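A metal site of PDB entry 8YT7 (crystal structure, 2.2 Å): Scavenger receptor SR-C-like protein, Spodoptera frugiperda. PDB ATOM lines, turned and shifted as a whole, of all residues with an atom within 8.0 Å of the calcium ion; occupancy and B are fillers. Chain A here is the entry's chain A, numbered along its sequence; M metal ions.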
ATOM      1  N   CYS A   5     -16.490  26.361  14.085  1.00  0.00           N
ATOM      2  CA  CYS A   5     -15.156  25.855  13.749  1.00  0.00           C
ATOM      3  C   CYS A   5     -15.025  24.388  14.090  1.00  0.00           C
ATOM      4  O   CYS A   5     -15.316  23.979  15.221  1.00  0.00           O
ATOM      5  CB  CYS A   5     -14.047  26.609  14.493  1.00  0.00           C
ATOM      6  SG  CYS A   5     -12.423  26.412  13.636  1.00  0.00           S
ATOM      7  N   ASP A   6     -14.557  23.611  13.108  1.00  0.00           N
ATOM      8  CA  ASP A   6     -14.255  22.202  13.291  1.00  0.00           C
ATOM      9  C   ASP A   6     -12.760  21.960  13.513  1.00  0.00           C
ATOM     10  O   ASP A   6     -12.359  20.800  13.698  1.00  0.00           O
ATOM     11  CB  ASP A   6     -14.763  21.389  12.094  1.00  0.00           C
ATOM     12  CG  ASP A   6     -14.201  21.895  10.763  1.00  0.00           C
ATOM     13  OD1 ASP A   6     -13.281  22.745  10.775  1.00  0.00           O
ATOM     14  OD2 ASP A   6     -14.671  21.434   9.688  1.00  0.00           O
ATOM     15  N   PHE A   7     -11.945  23.018  13.456  1.00  0.00           N
ATOM     16  CA  PHE A   7     -10.508  22.987  13.739  1.00  0.00           C
ATOM     17  C   PHE A   7      -9.711  22.160  12.757  1.00  0.00           C
ATOM     18  O   PHE A   7      -8.569  21.774  13.053  1.00  0.00           O
ATOM     19  CB  PHE A   7     -10.248  22.513  15.177  1.00  0.00           C
ATOM     20  CG  PHE A   7     -10.892  23.373  16.204  1.00  0.00           C
ATOM     21  CD1 PHE A   7     -10.445  24.667  16.422  1.00  0.00           C
ATOM     22  CD2 PHE A   7     -11.984  22.907  16.927  1.00  0.00           C
ATOM     23  CE1 PHE A   7     -11.048  25.492  17.356  1.00  0.00           C
ATOM     24  CE2 PHE A   7     -12.603  23.718  17.866  1.00  0.00           C
ATOM     25  CZ  PHE A   7     -12.118  25.030  18.083  1.00  0.00           C
ATOM     26  N   GLU A   8     -10.270  21.903  11.571  1.00  0.00           N
ATOM     27  CA  GLU A   8      -9.536  21.132  10.580  1.00  0.00           C
ATOM     28  C   GLU A   8      -8.427  21.945   9.935  1.00  0.00           C
ATOM     29  O   GLU A   8      -7.434  21.376   9.489  1.00  0.00           O
ATOM     30  CB  GLU A   8     -10.483  20.587   9.516  1.00  0.00           C
ATOM     31  CG  GLU A   8     -11.538  19.622  10.055  1.00  0.00           C
ATOM     32  CD  GLU A   8     -10.974  18.609  11.066  1.00  0.00           C
ATOM     33  OE1 GLU A   8      -9.955  17.950  10.752  1.00  0.00           O
ATOM     34  OE2 GLU A   8     -11.570  18.461  12.160  1.00  0.00           O
ATOM     35  N   LEU A   9      -8.560  23.269   9.896  1.00  0.00           N
ATOM     36  CA  LEU A   9      -7.493  24.049   9.300  1.00  0.00           C
ATOM     37  C   LEU A   9      -6.606  24.631  10.392  1.00  0.00           C
ATOM     38  O   LEU A   9      -7.055  24.824  11.530  1.00  0.00           O
ATOM     39  CB  LEU A   9      -8.058  25.195   8.435  1.00  0.00           C
ATOM     40  CG  LEU A   9      -8.705  24.925   7.070  1.00  0.00           C
ATOM     41  CD1 LEU A   9      -7.800  24.200   6.076  1.00  0.00           C
ATOM     42  CD2 LEU A   9     -10.069  24.257   7.205  1.00  0.00           C
ATOM     43  N   ARG A  27      -3.450  22.083  18.631  1.00  0.00           N
ATOM     44  CA  ARG A  27      -4.265  21.374  17.651  1.00  0.00           C
ATOM     45  C   ARG A  27      -3.618  20.025  17.398  1.00  0.00           C
ATOM     46  O   ARG A  27      -2.388  19.939  17.238  1.00  0.00           O
ATOM     47  CB  ARG A  27      -4.399  22.176  16.357  1.00  0.00           C
ATOM     48  CG  ARG A  27      -5.107  21.476  15.211  1.00  0.00           C
ATOM     49  CD  ARG A  27      -5.342  22.476  14.107  1.00  0.00           C
ATOM     50  NE  ARG A  27      -5.594  21.836  12.826  1.00  0.00           N
ATOM     51  CZ  ARG A  27      -4.673  21.546  11.916  1.00  0.00           C
ATOM     52  NH1 ARG A  27      -3.397  21.836  12.129  1.00  0.00           N
ATOM     53  NH2 ARG A  27      -5.052  20.959  10.799  1.00  0.00           N
ATOM     54  N   LEU A  28      -4.393  18.943  17.419  1.00  0.00           N
ATOM     55  CA  LEU A  28      -3.862  17.592  17.218  1.00  0.00           C
ATOM     56  C   LEU A  28      -4.809  16.635  16.550  1.00  0.00           C
ATOM     57  O   LEU A  28      -6.004  16.755  16.682  1.00  0.00           O
ATOM     58  CB  LEU A  28      -3.394  16.979  18.514  1.00  0.00           C
ATOM     59  CG  LEU A  28      -2.258  15.954  18.474  1.00  0.00           C
ATOM     60  CD1 LEU A  28      -0.950  16.630  18.127  1.00  0.00           C
ATOM     61  CD2 LEU A  28      -2.155  15.191  19.778  1.00  0.00           C
ATOM     62  N   ASN A  29      -4.242  15.631  15.904  1.00  0.00           N
ATOM     63  CA  ASN A  29      -5.020  14.688  15.149  1.00  0.00           C
ATOM     64  C   ASN A  29      -5.627  13.554  15.871  1.00  0.00           C
ATOM     65  O   ASN A  29      -6.820  13.477  15.962  1.00  0.00           O
ATOM     66  CB  ASN A  29      -4.151  14.087  14.064  1.00  0.00           C
ATOM     67  CG  ASN A  29      -4.947  13.307  13.064  1.00  0.00           C
ATOM     68  OD1 ASN A  29      -6.094  13.620  12.787  1.00  0.00           O
ATOM     69  ND2 ASN A  29      -4.335  12.290  12.512  1.00  0.00           N
ATOM     70  N   TYR A  43      -9.507  10.396  19.032  1.00  0.00           N
ATOM     71  CA  TYR A  43      -9.853  10.964  17.732  1.00  0.00           C
ATOM     72  C   TYR A  43     -10.774  12.147  17.985  1.00  0.00           C
ATOM     73  O   TYR A  43     -11.336  12.288  19.077  1.00  0.00           O
ATOM     74  CB  TYR A  43     -10.545   9.930  16.829  1.00  0.00           C
ATOM     75  CG  TYR A  43     -11.548   9.093  17.601  1.00  0.00           C
ATOM     76  CD1 TYR A  43     -12.809   9.609  17.925  1.00  0.00           C
ATOM     77  CD2 TYR A  43     -11.243   7.812  18.014  1.00  0.00           C
ATOM     78  CE1 TYR A  43     -13.727   8.852  18.645  1.00  0.00           C
ATOM     79  CE2 TYR A  43     -12.163   7.042  18.730  1.00  0.00           C
ATOM     80  CZ  TYR A  43     -13.399   7.581  19.042  1.00  0.00           C
ATOM     81  OH  TYR A  43     -14.298   6.855  19.752  1.00  0.00           O
ATOM     82  N   ASP A  44     -10.953  13.000  16.966  1.00  0.00           N
ATOM     83  CA  ASP A  44     -11.741  14.200  17.162  1.00  0.00           C
ATOM     84  C   ASP A  44     -13.225  13.886  17.061  1.00  0.00           C
ATOM     85  O   ASP A  44     -13.632  12.756  16.782  1.00  0.00           O
ATOM     86  CB  ASP A  44     -11.378  15.303  16.148  1.00  0.00           C
ATOM     87  CG  ASP A  44     -12.011  15.077  14.756  1.00  0.00           C
ATOM     88  OD1 ASP A  44     -12.540  13.984  14.457  1.00  0.00           O
ATOM     89  OD2 ASP A  44     -12.064  16.082  14.004  1.00  0.00           O
ATOM     90  N   HIS A  45     -14.066  14.906  17.229  1.00  0.00           N
ATOM     91  CA  HIS A  45     -15.488  14.654  17.027  1.00  0.00           C
ATOM     92  C   HIS A  45     -15.919  14.826  15.575  1.00  0.00           C
ATOM     93  O   HIS A  45     -16.831  14.127  15.138  1.00  0.00           O
ATOM     94  CB  HIS A  45     -16.332  15.576  17.898  1.00  0.00           C
ATOM     95  CG  HIS A  45     -17.792  15.286  17.828  1.00  0.00           C
ATOM     96  ND1 HIS A  45     -18.661  16.025  17.044  1.00  0.00           N
ATOM     97  CD2 HIS A  45     -18.531  14.296  18.385  1.00  0.00           C
ATOM     98  CE1 HIS A  45     -19.873  15.511  17.155  1.00  0.00           C
ATOM     99  NE2 HIS A  45     -19.827  14.474  17.960  1.00  0.00           N
ATOM    100  N   THR A  46     -15.289  15.713  14.820  1.00  0.00           N
ATOM    101  CA  THR A  46     -15.793  16.007  13.485  1.00  0.00           C
ATOM    102  C   THR A  46     -15.861  14.747  12.614  1.00  0.00           C
ATOM    103  O   THR A  46     -16.902  14.420  12.051  1.00  0.00           O
ATOM    104  CB  THR A  46     -14.940  17.067  12.801  1.00  0.00           C
ATOM    105  OG1 THR A  46     -14.907  18.263  13.608  1.00  0.00           O
ATOM    106  CG2 THR A  46     -15.572  17.416  11.463  1.00  0.00           C
ATOM    107  N   TYR A  47     -14.753  14.017  12.506  1.00  0.00           N
ATOM    108  CA  TYR A  47     -14.676  12.828  11.658  1.00  0.00           C
ATOM    109  C   TYR A  47     -14.703  11.515  12.444  1.00  0.00           C
ATOM    110  O   TYR A  47     -14.752  10.456  11.826  1.00  0.00           O
ATOM    111  CB  TYR A  47     -13.421  12.889  10.778  1.00  0.00           C
ATOM    112  CG  TYR A  47     -13.463  14.009   9.759  1.00  0.00           C
ATOM    113  CD1 TYR A  47     -14.276  13.938   8.632  1.00  0.00           C
ATOM    114  CD2 TYR A  47     -12.694  15.144   9.922  1.00  0.00           C
ATOM    115  CE1 TYR A  47     -14.306  14.965   7.710  1.00  0.00           C
ATOM    116  CE2 TYR A  47     -12.710  16.166   9.010  1.00  0.00           C
ATOM    117  CZ  TYR A  47     -13.514  16.068   7.918  1.00  0.00           C
ATOM    118  OH  TYR A  47     -13.536  17.108   7.022  1.00  0.00           O
ATOM    119  N   GLY A  48     -14.679  11.569  13.776  1.00  0.00           N
ATOM    120  CA  GLY A  48     -14.921  10.428  14.651  1.00  0.00           C
ATOM    121  C   GLY A  48     -13.900   9.315  14.490  1.00  0.00           C
ATOM    122  O   GLY A  48     -12.775   9.521  14.024  1.00  0.00           O
ATOM    123  N   SER A  52      -8.935  10.602  11.588  1.00  0.00           N
ATOM    124  CA  SER A  52      -7.892  11.589  11.286  1.00  0.00           C
ATOM    125  C   SER A  52      -8.402  13.036  11.276  1.00  0.00           C
ATOM    126  O   SER A  52      -7.871  13.878  10.541  1.00  0.00           O
ATOM    127  CB  SER A  52      -7.188  11.280   9.964  1.00  0.00           C
ATOM    128  OG  SER A  52      -6.191  10.288  10.133  1.00  0.00           O
ATOM    129  N   GLY A  53      -9.399  13.368  12.088  1.00  0.00           N
ATOM    130  CA  GLY A  53      -9.810  14.748  12.244  1.00  0.00           C
ATOM    131  C   GLY A  53      -9.160  15.400  13.445  1.00  0.00           C
ATOM    132  O   GLY A  53      -8.667  14.713  14.331  1.00  0.00           O
ATOM    133  N   TYR A  54      -9.211  16.729  13.498  1.00  0.00           N
ATOM    134  CA  TYR A  54      -8.433  17.517  14.457  1.00  0.00           C
ATOM    135  C   TYR A  54      -9.286  18.083  15.574  1.00  0.00           C
ATOM    136  O   TYR A  54     -10.367  18.620  15.341  1.00  0.00           O
ATOM    137  CB  TYR A  54      -7.728  18.696  13.767  1.00  0.00           C
ATOM    138  CG  TYR A  54      -6.558  18.271  12.940  1.00  0.00           C
ATOM    139  CD1 TYR A  54      -6.723  17.881  11.618  1.00  0.00           C
ATOM    140  CD2 TYR A  54      -5.283  18.228  13.490  1.00  0.00           C
ATOM    141  CE1 TYR A  54      -5.636  17.494  10.848  1.00  0.00           C
ATOM    142  CE2 TYR A  54      -4.205  17.830  12.737  1.00  0.00           C
ATOM    143  CZ  TYR A  54      -4.381  17.468  11.423  1.00  0.00           C
ATOM    144  OH  TYR A  54      -3.282  17.070  10.683  1.00  0.00           O
ATOM    145  N   TYR A  55      -8.748  18.054  16.795  1.00  0.00           N
ATOM    146  CA  TYR A  55      -9.351  18.724  17.933  1.00  0.00           C
ATOM    147  C   TYR A  55      -8.333  19.667  18.571  1.00  0.00           C
ATOM    148  O   TYR A  55      -7.143  19.705  18.205  1.00  0.00           O
ATOM    149  CB  TYR A  55      -9.826  17.688  18.948  1.00  0.00           C
ATOM    150  CG  TYR A  55      -8.756  16.697  19.292  1.00  0.00           C
ATOM    151  CD1 TYR A  55      -7.764  17.018  20.196  1.00  0.00           C
ATOM    152  CD2 TYR A  55      -8.711  15.449  18.686  1.00  0.00           C
ATOM    153  CE1 TYR A  55      -6.778  16.137  20.514  1.00  0.00           C
ATOM    154  CE2 TYR A  55      -7.715  14.536  19.005  1.00  0.00           C
ATOM    155  CZ  TYR A  55      -6.745  14.901  19.921  1.00  0.00           C
ATOM    156  OH  TYR A  55      -5.721  14.042  20.270  1.00  0.00           O
ATOM    157  N   MET A  56      -8.782  20.431  19.561  1.00  0.00           N
ATOM    158  CA  MET A  56      -7.891  21.193  20.416  1.00  0.00           C
ATOM    159  C   MET A  56      -7.814  20.561  21.790  1.00  0.00           C
ATOM    160  O   MET A  56      -8.793  20.031  22.293  1.00  0.00           O
ATOM    161  CB  MET A  56      -8.316  22.665  20.526  1.00  0.00           C
ATOM    162  CG  MET A  56      -8.565  23.339  19.162  1.00  0.00           C
ATOM    163  SD  MET A  56      -7.016  23.719  18.311  1.00  0.00           S
ATOM    164  CE  MET A  56      -6.098  24.703  19.510  1.00  0.00           C
ATOM    165  N   TRP A 136     -16.742  11.519  23.986  1.00  0.00           N
ATOM    166  CA  TRP A 136     -17.086  12.880  23.595  1.00  0.00           C
ATOM    167  C   TRP A 136     -18.490  13.229  24.075  1.00  0.00           C
ATOM    168  O   TRP A 136     -19.477  12.573  23.698  1.00  0.00           O
ATOM    169  CB  TRP A 136     -16.997  13.029  22.073  1.00  0.00           C
ATOM    170  CG  TRP A 136     -15.596  13.155  21.561  1.00  0.00           C
ATOM    171  CD1 TRP A 136     -14.803  12.164  21.063  1.00  0.00           C
ATOM    172  CD2 TRP A 136     -14.811  14.355  21.515  1.00  0.00           C
ATOM    173  NE1 TRP A 136     -13.567  12.682  20.703  1.00  0.00           N
ATOM    174  CE2 TRP A 136     -13.560  14.016  20.973  1.00  0.00           C
ATOM    175  CE3 TRP A 136     -15.051  15.677  21.877  1.00  0.00           C
ATOM    176  CZ2 TRP A 136     -12.556  14.956  20.789  1.00  0.00           C
ATOM    177  CZ3 TRP A 136     -14.057  16.598  21.686  1.00  0.00           C
ATOM    178  CH2 TRP A 136     -12.825  16.231  21.144  1.00  0.00           C
ATOM    179  N   ILE A 168     -11.529  19.917  23.028  1.00  0.00           N
ATOM    180  CA  ILE A 168     -12.737  20.476  22.454  1.00  0.00           C
ATOM    181  C   ILE A 168     -12.697  20.279  20.957  1.00  0.00           C
ATOM    182  O   ILE A 168     -11.642  20.060  20.353  1.00  0.00           O
ATOM    183  CB  ILE A 168     -12.909  21.968  22.770  1.00  0.00           C
ATOM    184  CG1 ILE A 168     -11.705  22.712  22.183  1.00  0.00           C
ATOM    185  CG2 ILE A 168     -12.988  22.190  24.251  1.00  0.00           C
ATOM    186  CD1 ILE A 168     -11.864  24.171  22.205  1.00  0.00           C
ATOM    187  N   ASP A 169     -13.895  20.354  20.370  1.00  0.00           N
ATOM    188  CA  ASP A 169     -14.105  20.229  18.938  1.00  0.00           C
ATOM    189  C   ASP A 169     -15.494  20.787  18.624  1.00  0.00           C
ATOM    190  O   ASP A 169     -16.345  20.956  19.512  1.00  0.00           O
ATOM    191  CB  ASP A 169     -13.959  18.766  18.473  1.00  0.00           C
ATOM    192  CG  ASP A 169     -13.526  18.629  17.004  1.00  0.00           C
ATOM    193  OD1 ASP A 169     -13.310  19.628  16.303  1.00  0.00           O
ATOM    194  OD2 ASP A 169     -13.408  17.477  16.560  1.00  0.00           O
ATOM    195  N   ASP A 170     -15.674  21.117  17.347  1.00  0.00           N
ATOM    196  CA  ASP A 170     -16.957  21.440  16.746  1.00  0.00           C
ATOM    197  C   ASP A 170     -17.715  22.498  17.552  1.00  0.00           C
ATOM    198  O   ASP A 170     -18.760  22.234  18.143  1.00  0.00           O
ATOM    199  CB  ASP A 170     -17.782  20.157  16.575  1.00  0.00           C
ATOM    200  CG  ASP A 170     -17.230  19.247  15.505  1.00  0.00           C
ATOM    201  OD1 ASP A 170     -16.500  19.737  14.623  1.00  0.00           O
ATOM    202  OD2 ASP A 170     -17.523  18.030  15.522  1.00  0.00           O
ATOM    203  N   VAL A 171     -17.152  23.713  17.576  1.00  0.00           N
ATOM    204  CA  VAL A 171     -17.787  24.812  18.299  1.00  0.00           C
ATOM    205  C   VAL A 171     -18.730  25.541  17.370  1.00  0.00           C
ATOM    206  O   VAL A 171     -18.633  25.466  16.146  1.00  0.00           O
ATOM    207  CB  VAL A 171     -16.751  25.775  18.913  1.00  0.00           C
ATOM    208  CG1 VAL A 171     -15.799  25.000  19.798  1.00  0.00           C
ATOM    209  CG2 VAL A 171     -16.022  26.516  17.805  1.00  0.00           C
HETATM  210 CA    CA M   1     -12.508  18.506  14.420  1.00  0.00          CA
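OD1 of Asp 44 sits at hydrogen-bond distance from N of Gly 48 (3.3 Å).
The side-chain carboxylate (OD2) of Asp 169 lies close to the backbone NH (N) of His 45, 2.7 Å away.
The side-chain carboxylate of Asp 170 lies within hydrogen-bond range of the backbone NH of Thr 46 (3.3 Å).
OD1 of Asp 44 lies within hydrogen-bond range of N of Tyr 47, at 3.0 Å.
O of Glu 8 sits at hydrogen-bond distance from NH2 of Arg 27, 2.8 Å away.
Six residues have an atom within 4 Å of the calcium ion: Asp 6, Glu 8, Asp 44, Thr 46, Tyr 54 and Asp 169.
The nearest printed residue that does not touch the calcium ion is Asp 170 (4.2 Å).
The calcium ion is bound by the backbone carbonyl oxygen (O) of Tyr 54 (2.3 Å), the side-chain carboxylate (OD1) of Asp 169 (2.3 Å), the backbone carbonyl oxygen (O) of Asp 6 (2.4 Å), the side-chain carboxylate (OE2) of Glu 8 (2.4 Å), the side-chain carboxylate (OD2) of Asp 44 (2.5 Å), the side-chain carboxylate (OD2) of Asp 169 (2.5 Å) and the side-chain hydroxyl (OG1) of Thr 46 (2.5 Å).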
